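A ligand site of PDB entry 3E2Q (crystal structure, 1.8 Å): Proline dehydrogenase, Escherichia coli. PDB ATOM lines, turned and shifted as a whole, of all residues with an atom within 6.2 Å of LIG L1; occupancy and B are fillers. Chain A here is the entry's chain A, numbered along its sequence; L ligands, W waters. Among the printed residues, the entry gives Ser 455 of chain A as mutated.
The guanidinium group (NH1) of Arg 470 lies within salt-bridge range of the side-chain carboxylate (OE2) of Glu 204 (2.8 Å). NE of Arg 471 lies within salt-bridge range of OE1 of Glu 474 (2.9 Å). The side-chain amino group of Lys 244 lies within salt-bridge range of the side-chain carboxylate of Asp 285, 3.0 Å away.
Water W1 lies within hydrogen-bond range of OH of Tyr 352, N1 of LIG L1, O of Ala 286, NZ of Lys 244 and O8 of LG2 L2. Water W3 lies within hydrogen-bond range of OD1 of Asp 285, NH1 of Arg 346, N8 of LG2 L2 and O2 of LIG L1. Water W2 lies within hydrogen-bond range of OG of Ser 455 (2.5 Å), OD2 of Asp 200 (2.8 Å) and OH of Tyr 467 (2.9 Å).
An oxygen (O1) of LIG L1 is in salt-bridge range of the guanidinium group (NH1) of Arg 471. OG of Ser 455 is in hydrogen-bond range of O2 of LIG L1, 3.1 Å away. O of Ala 286 is in hydrogen-bond range of N7 of LG2 L2 (2.7 Å). O8 of LG2 L2 lies within hydrogen-bond range of N of Ala 286 (2.9 Å). NZ of Lys 244 is in salt-bridge range of O3 of LIG L1 (3.0 Å). The guanidinium group of Arg 470 is in salt-bridge range of an oxygen (O3) of LIG L1. The backbone NH (N) of Ala 351 is in hydrogen-bond range of an oxygen (O7) of LG2 L2, 2.8 Å away. OE2 of Glu 474 lies within hydrogen-bond range of O10 of LG2 L2, 2.7 Å away. OD2 of Asp 285 is in salt-bridge range of N1 of LIG L1.
OD2 of Asp 200 touches C4 of LIG L1 (3.4 Å). Ala 351 touches LIG L1 (CB to O1, 3.8 Å). Leu 428 touches LIG L1. Tyr 467 touches LIG L1. Hydrophobic or aromatic side chains within 4 Å of LIG L1: Ala 351, Leu 428 and Tyr 467. Nine residues have an atom within 4 Å of LIG L1: Asp 200, Lys 244, Asp 285, Ala 351, Leu 428, Ser 455, Tyr 467, Arg 470 and Arg 471.
N1 of LIG L1 sits close to N8 of LG2 L2 (3.3 Å).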
ATOM      1  N   ASP A 200       3.816  25.194 -14.028  1.00  0.00           N
ATOM      2  CA  ASP A 200       3.920  24.088 -13.088  1.00  0.00           C
ATOM      3  C   ASP A 200       4.167  22.823 -13.874  1.00  0.00           C
ATOM      4  O   ASP A 200       3.234  22.214 -14.397  1.00  0.00           O
ATOM      5  CB  ASP A 200       2.610  23.989 -12.299  1.00  0.00           C
ATOM      6  CG  ASP A 200       2.516  22.744 -11.438  1.00  0.00           C
ATOM      7  OD1 ASP A 200       3.542  22.034 -11.277  1.00  0.00           O
ATOM      8  OD2 ASP A 200       1.409  22.472 -10.927  1.00  0.00           O
ATOM      9  N   GLU A 204       5.981  14.427 -10.002  1.00  0.00           N
ATOM     10  CA  GLU A 204       6.450  14.611  -8.636  1.00  0.00           C
ATOM     11  C   GLU A 204       6.817  13.273  -8.038  1.00  0.00           C
ATOM     12  O   GLU A 204       6.558  12.230  -8.640  1.00  0.00           O
ATOM     13  CB  GLU A 204       5.344  15.278  -7.804  1.00  0.00           C
ATOM     14  CG  GLU A 204       4.047  14.492  -7.781  1.00  0.00           C
ATOM     15  CD  GLU A 204       2.890  15.306  -7.241  1.00  0.00           C
ATOM     16  OE1 GLU A 204       2.418  16.232  -7.939  1.00  0.00           O
ATOM     17  OE2 GLU A 204       2.443  14.996  -6.112  1.00  0.00           O
ATOM     18  N   SER A 242       7.467  27.052 -11.217  1.00  0.00           N
ATOM     19  CA  SER A 242       7.408  26.481  -9.886  1.00  0.00           C
ATOM     20  C   SER A 242       7.969  25.080  -9.935  1.00  0.00           C
ATOM     21  O   SER A 242       7.823  24.356 -10.929  1.00  0.00           O
ATOM     22  CB  SER A 242       5.968  26.458  -9.340  1.00  0.00           C
ATOM     23  OG  SER A 242       5.122  25.721 -10.197  1.00  0.00           O
ATOM     24  N   LYS A 244       8.907  21.268  -7.721  1.00  0.00           N
ATOM     25  CA  LYS A 244       8.685  20.424  -6.562  1.00  0.00           C
ATOM     26  C   LYS A 244       9.990  19.759  -6.201  1.00  0.00           C
ATOM     27  O   LYS A 244      10.628  19.104  -7.038  1.00  0.00           O
ATOM     28  CB  LYS A 244       7.623  19.367  -6.871  1.00  0.00           C
ATOM     29  CG  LYS A 244       6.206  19.900  -6.735  1.00  0.00           C
ATOM     30  CD  LYS A 244       5.187  18.834  -7.054  1.00  0.00           C
ATOM     31  CE  LYS A 244       3.805  19.201  -6.543  1.00  0.00           C
ATOM     32  NZ  LYS A 244       3.292  20.395  -7.245  1.00  0.00           N
ATOM     33  N   ASP A 285       7.482  24.767  -4.426  1.00  0.00           N
ATOM     34  CA  ASP A 285       6.174  24.284  -3.989  1.00  0.00           C
ATOM     35  C   ASP A 285       6.263  23.642  -2.607  1.00  0.00           C
ATOM     36  O   ASP A 285       7.303  23.108  -2.241  1.00  0.00           O
ATOM     37  CB  ASP A 285       5.631  23.226  -4.961  1.00  0.00           C
ATOM     38  CG  ASP A 285       5.083  23.824  -6.234  1.00  0.00           C
ATOM     39  OD1 ASP A 285       5.067  25.059  -6.382  1.00  0.00           O
ATOM     40  OD2 ASP A 285       4.666  23.023  -7.108  1.00  0.00           O
ATOM     41  N   ALA A 286       5.157  23.712  -1.859  1.00  0.00           N
ATOM     42  CA  ALA A 286       5.054  23.022  -0.584  1.00  0.00           C
ATOM     43  C   ALA A 286       4.325  21.704  -0.799  1.00  0.00           C
ATOM     44  O   ALA A 286       3.299  21.643  -1.475  1.00  0.00           O
ATOM     45  CB  ALA A 286       4.305  23.872   0.426  1.00  0.00           C
ATOM     46  N   ARG A 346       4.196  32.536  -1.580  1.00  0.00           N
ATOM     47  CA  ARG A 346       2.832  32.132  -1.910  1.00  0.00           C
ATOM     48  C   ARG A 346       2.161  31.580  -0.684  1.00  0.00           C
ATOM     49  O   ARG A 346       2.557  30.542  -0.169  1.00  0.00           O
ATOM     50  CB  ARG A 346       2.848  31.056  -2.995  1.00  0.00           C
ATOM     51  CG  ARG A 346       3.471  31.554  -4.282  1.00  0.00           C
ATOM     52  CD  ARG A 346       3.413  30.483  -5.356  1.00  0.00           C
ATOM     53  NE  ARG A 346       4.071  30.947  -6.574  1.00  0.00           N
ATOM     54  CZ  ARG A 346       4.037  30.282  -7.721  1.00  0.00           C
ATOM     55  NH1 ARG A 346       3.373  29.125  -7.797  1.00  0.00           N
ATOM     56  NH2 ARG A 346       4.652  30.787  -8.786  1.00  0.00           N
ATOM     57  N   ALA A 351      -2.965  21.613  -0.195  1.00  0.00           N
ATOM     58  CA  ALA A 351      -3.587  20.703  -1.153  1.00  0.00           C
ATOM     59  C   ALA A 351      -3.620  19.254  -0.718  1.00  0.00           C
ATOM     60  O   ALA A 351      -4.200  18.413  -1.404  1.00  0.00           O
ATOM     61  CB  ALA A 351      -2.878  20.841  -2.531  1.00  0.00           C
ATOM     62  N   TYR A 352      -3.016  18.950   0.426  1.00  0.00           N
ATOM     63  CA  TYR A 352      -2.848  17.547   0.821  1.00  0.00           C
ATOM     64  C   TYR A 352      -3.608  17.154   2.078  1.00  0.00           C
ATOM     65  O   TYR A 352      -3.210  16.216   2.764  1.00  0.00           O
ATOM     66  CB  TYR A 352      -1.368  17.252   1.050  1.00  0.00           C
ATOM     67  CG  TYR A 352      -0.482  17.610  -0.123  1.00  0.00           C
ATOM     68  CD1 TYR A 352      -0.059  16.634  -1.014  1.00  0.00           C
ATOM     69  CD2 TYR A 352      -0.058  18.915  -0.324  1.00  0.00           C
ATOM     70  CE1 TYR A 352       0.767  16.967  -2.097  1.00  0.00           C
ATOM     71  CE2 TYR A 352       0.765  19.254  -1.394  1.00  0.00           C
ATOM     72  CZ  TYR A 352       1.175  18.276  -2.280  1.00  0.00           C
ATOM     73  OH  TYR A 352       1.975  18.647  -3.338  1.00  0.00           O
ATOM     74  N   LEU A 428      -5.387  28.651  -9.705  1.00  0.00           N
ATOM     75  CA  LEU A 428      -5.071  27.500 -10.544  1.00  0.00           C
ATOM     76  C   LEU A 428      -5.841  27.601 -11.842  1.00  0.00           C
ATOM     77  O   LEU A 428      -7.029  27.924 -11.845  1.00  0.00           O
ATOM     78  CB  LEU A 428      -5.469  26.189  -9.841  1.00  0.00           C
ATOM     79  CG  LEU A 428      -4.790  25.911  -8.509  1.00  0.00           C
ATOM     80  CD1 LEU A 428      -5.252  24.568  -7.933  1.00  0.00           C
ATOM     81  CD2 LEU A 428      -3.269  25.931  -8.696  1.00  0.00           C
ATOM     82  N   SER A 455      -1.401  29.630 -12.048  1.00  0.00           N
ATOM     83  CA  SER A 455      -0.529  28.463 -12.068  1.00  0.00           C
ATOM     84  C   SER A 455      -1.009  27.528 -13.177  1.00  0.00           C
ATOM     85  O   SER A 455      -2.158  27.081 -13.177  1.00  0.00           O
ATOM     86  CB  SER A 455      -0.542  27.750 -10.714  1.00  0.00           C
ATOM     87  OG  SER A 455       0.335  26.632 -10.722  1.00  0.00           O
ATOM     88  N   TYR A 467      -1.670  15.353  -9.393  1.00  0.00           N
ATOM     89  CA  TYR A 467      -2.242  16.697  -9.465  1.00  0.00           C
ATOM     90  C   TYR A 467      -3.762  16.617  -9.645  1.00  0.00           C
ATOM     91  O   TYR A 467      -4.531  17.316  -8.977  1.00  0.00           O
ATOM     92  CB  TYR A 467      -1.591  17.481 -10.619  1.00  0.00           C
ATOM     93  CG  TYR A 467      -1.995  18.941 -10.689  1.00  0.00           C
ATOM     94  CD1 TYR A 467      -1.268  19.912 -10.012  1.00  0.00           C
ATOM     95  CD2 TYR A 467      -3.095  19.332 -11.435  1.00  0.00           C
ATOM     96  CE1 TYR A 467      -1.628  21.254 -10.077  1.00  0.00           C
ATOM     97  CE2 TYR A 467      -3.470  20.686 -11.494  1.00  0.00           C
ATOM     98  CZ  TYR A 467      -2.735  21.637 -10.822  1.00  0.00           C
ATOM     99  OH  TYR A 467      -3.100  22.957 -10.887  1.00  0.00           O
ATOM    100  N   ARG A 470      -5.600  15.609  -6.476  1.00  0.00           N
ATOM    101  CA  ARG A 470      -5.714  16.732  -5.552  1.00  0.00           C
ATOM    102  C   ARG A 470      -6.808  17.716  -5.998  1.00  0.00           C
ATOM    103  O   ARG A 470      -7.537  18.247  -5.166  1.00  0.00           O
ATOM    104  CB  ARG A 470      -4.361  17.453  -5.354  1.00  0.00           C
ATOM    105  CG  ARG A 470      -3.371  16.600  -4.557  1.00  0.00           C
ATOM    106  CD  ARG A 470      -2.146  17.392  -4.122  1.00  0.00           C
ATOM    107  NE  ARG A 470      -1.369  17.891  -5.246  1.00  0.00           N
ATOM    108  CZ  ARG A 470      -0.390  17.218  -5.849  1.00  0.00           C
ATOM    109  NH1 ARG A 470      -0.070  15.994  -5.450  1.00  0.00           N
ATOM    110  NH2 ARG A 470       0.251  17.790  -6.864  1.00  0.00           N
ATOM    111  N   ARG A 471      -6.920  17.938  -7.308  1.00  0.00           N
ATOM    112  CA  ARG A 471      -7.979  18.805  -7.823  1.00  0.00           C
ATOM    113  C   ARG A 471      -9.364  18.201  -7.614  1.00  0.00           C
ATOM    114  O   ARG A 471     -10.323  18.925  -7.332  1.00  0.00           O
ATOM    115  CB  ARG A 471      -7.770  19.104  -9.320  1.00  0.00           C
ATOM    116  CG  ARG A 471      -6.440  19.783  -9.651  1.00  0.00           C
ATOM    117  CD  ARG A 471      -6.404  21.223  -9.180  1.00  0.00           C
ATOM    118  NE  ARG A 471      -6.114  21.389  -7.750  1.00  0.00           N
ATOM    119  CZ  ARG A 471      -4.928  21.130  -7.193  1.00  0.00           C
ATOM    120  NH1 ARG A 471      -3.938  20.633  -7.928  1.00  0.00           N
ATOM    121  NH2 ARG A 471      -4.748  21.346  -5.896  1.00  0.00           N
ATOM    122  N   GLU A 474     -10.227  18.730  -3.969  1.00  0.00           N
ATOM    123  CA  GLU A 474     -10.454  20.163  -3.756  1.00  0.00           C
ATOM    124  C   GLU A 474     -11.831  20.551  -4.295  1.00  0.00           C
ATOM    125  O   GLU A 474     -12.619  21.218  -3.611  1.00  0.00           O
ATOM    126  CB  GLU A 474      -9.355  20.966  -4.447  1.00  0.00           C
ATOM    127  CG  GLU A 474      -9.322  22.452  -4.058  1.00  0.00           C
ATOM    128  CD  GLU A 474      -8.279  23.226  -4.836  1.00  0.00           C
ATOM    129  OE1 GLU A 474      -7.416  22.599  -5.495  1.00  0.00           O
ATOM    130  OE2 GLU A 474      -8.299  24.485  -4.783  1.00  0.00           O
HETATM  131  N1  LIG L   1       1.153  22.997  -6.134  1.00  0.00           N
HETATM  132  C1  LIG L   1      -0.229  22.734  -6.181  1.00  0.00           C
HETATM  133  C2  LIG L   1      -0.498  21.323  -6.330  1.00  0.00           C
HETATM  134  O1  LIG L   1      -1.564  20.878  -6.060  1.00  0.00           O
HETATM  135  C3  LIG L   1      -0.782  23.516  -7.273  1.00  0.00           C
HETATM  136  C4  LIG L   1       0.351  23.893  -8.016  1.00  0.00           C
HETATM  137  C5  LIG L   1       1.477  23.167  -7.550  1.00  0.00           C
HETATM  138  O2  LIG L   1       0.571  25.263  -7.980  1.00  0.00           O
HETATM  139  O3  LIG L   1       0.361  20.597  -6.722  1.00  0.00           O
HETATM  140  P1  LG2 L   2     -11.301  27.145   0.172  1.00  0.00           P
HETATM  141  O1  LG2 L   2     -12.599  26.277  -0.336  1.00  0.00           O
HETATM  142  O2  LG2 L   2     -11.680  28.391   0.839  1.00  0.00           O
HETATM  143  O3  LG2 L   2     -10.382  26.275   1.163  1.00  0.00           O
HETATM  144  C1  LG2 L   2     -10.031  25.013   0.661  1.00  0.00           C
HETATM  145  C2  LG2 L   2      -9.290  24.129   1.629  1.00  0.00           C
HETATM  146  O4  LG2 L   2      -9.296  24.254   3.042  1.00  0.00           O
HETATM  147  C3  LG2 L   2      -8.423  23.058   1.302  1.00  0.00           C
HETATM  148  O5  LG2 L   2      -7.845  22.940   0.035  1.00  0.00           O
HETATM  149  C4  LG2 L   2      -7.694  22.838   2.497  1.00  0.00           C
HETATM  150  O6  LG2 L   2      -6.379  23.347   2.584  1.00  0.00           O
HETATM  151  C5  LG2 L   2      -8.623  23.146   3.528  1.00  0.00           C
HETATM  152  N1  LG2 L   2      -9.461  22.194   4.234  1.00  0.00           N
HETATM  153  C6  LG2 L   2     -10.439  21.484   3.678  1.00  0.00           C
HETATM  154  N2  LG2 L   2     -11.059  20.770   4.694  1.00  0.00           N
HETATM  155  C7  LG2 L   2     -10.425  21.067   5.866  1.00  0.00           C
HETATM  156  C8  LG2 L   2     -10.612  20.667   7.159  1.00  0.00           C
HETATM  157  N3  LG2 L   2     -11.690  19.732   7.501  1.00  0.00           N
HETATM  158  N4  LG2 L   2      -9.842  21.133   8.123  1.00  0.00           N
HETATM  159  C9  LG2 L   2      -8.853  22.022   7.849  1.00  0.00           C
HETATM  160  N5  LG2 L   2      -8.675  22.419   6.571  1.00  0.00           N
HETATM  161  C10 LG2 L   2      -9.437  21.971   5.593  1.00  0.00           C
HETATM  162  N6  LG2 L   2      -1.147  23.776  -2.172  1.00  0.00           N
HETATM  163  C11 LG2 L   2      -0.130  23.095  -1.634  1.00  0.00           C
HETATM  164  O7  LG2 L   2      -0.303  22.305  -0.523  1.00  0.00           O
HETATM  165  N7  LG2 L   2       1.180  23.300  -2.019  1.00  0.00           N
HETATM  166  C12 LG2 L   2       1.430  24.225  -3.009  1.00  0.00           C
HETATM  167  O8  LG2 L   2       2.746  24.336  -3.395  1.00  0.00           O
HETATM  168  C13 LG2 L   2       0.414  24.932  -3.589  1.00  0.00           C
HETATM  169  N8  LG2 L   2       0.662  25.849  -4.568  1.00  0.00           N
HETATM  170  C14 LG2 L   2      -0.333  26.538  -5.105  1.00  0.00           C
HETATM  171  C15 LG2 L   2      -0.141  27.507  -6.088  1.00  0.00           C
HETATM  172  C16 LG2 L   2      -1.238  28.186  -6.613  1.00  0.00           C
HETATM  173  C17 LG2 L   2      -1.025  29.274  -7.671  1.00  0.00           C
HETATM  174  C18 LG2 L   2      -2.521  27.926  -6.167  1.00  0.00           C
HETATM  175  C19 LG2 L   2      -3.725  28.694  -6.694  1.00  0.00           C
HETATM  176  C20 LG2 L   2      -2.711  26.970  -5.173  1.00  0.00           C
HETATM  177  C21 LG2 L   2      -1.603  26.303  -4.673  1.00  0.00           C
HETATM  178  N9  LG2 L   2      -1.837  25.416  -3.742  1.00  0.00           N
HETATM  179  C22 LG2 L   2      -0.868  24.700  -3.185  1.00  0.00           C
HETATM  180  C23 LG2 L   2      -3.231  25.137  -3.676  1.00  0.00           C
HETATM  181  C24 LG2 L   2      -4.002  25.016  -2.422  1.00  0.00           C
HETATM  182  O9  LG2 L   2      -3.477  24.691  -1.399  1.00  0.00           O
HETATM  183  C25 LG2 L   2      -5.482  24.860  -2.757  1.00  0.00           C
HETATM  184  O10 LG2 L   2      -5.818  25.392  -4.030  1.00  0.00           O
HETATM  185  C26 LG2 L   2      -6.234  25.533  -1.651  1.00  0.00           C
HETATM  186  O11 LG2 L   2      -6.044  24.952  -0.395  1.00  0.00           O
HETATM  187  C27 LG2 L   2      -7.613  26.054  -2.002  1.00  0.00           C
HETATM  188  O12 LG2 L   2      -7.944  27.094  -1.145  1.00  0.00           O
HETATM  189  P2  LG2 L   2      -9.122  28.117  -1.518  1.00  0.00           P
HETATM  190  O13 LG2 L   2      -9.066  29.439  -0.563  1.00  0.00           O
HETATM  191  O14 LG2 L   2      -9.170  28.341  -2.954  1.00  0.00           O
HETATM  192  O15 LG2 L   2     -10.521  27.260  -1.249  1.00  0.00           O
HETATM  193  O   HOH W   1       2.471  21.234  -4.311  1.00  0.00           O
HETATM  194  O   HOH W   2      -0.623  24.380 -11.301  1.00  0.00           O
HETATM  195  O   HOH W   3       2.975  26.638  -6.355  1.00  0.00           O
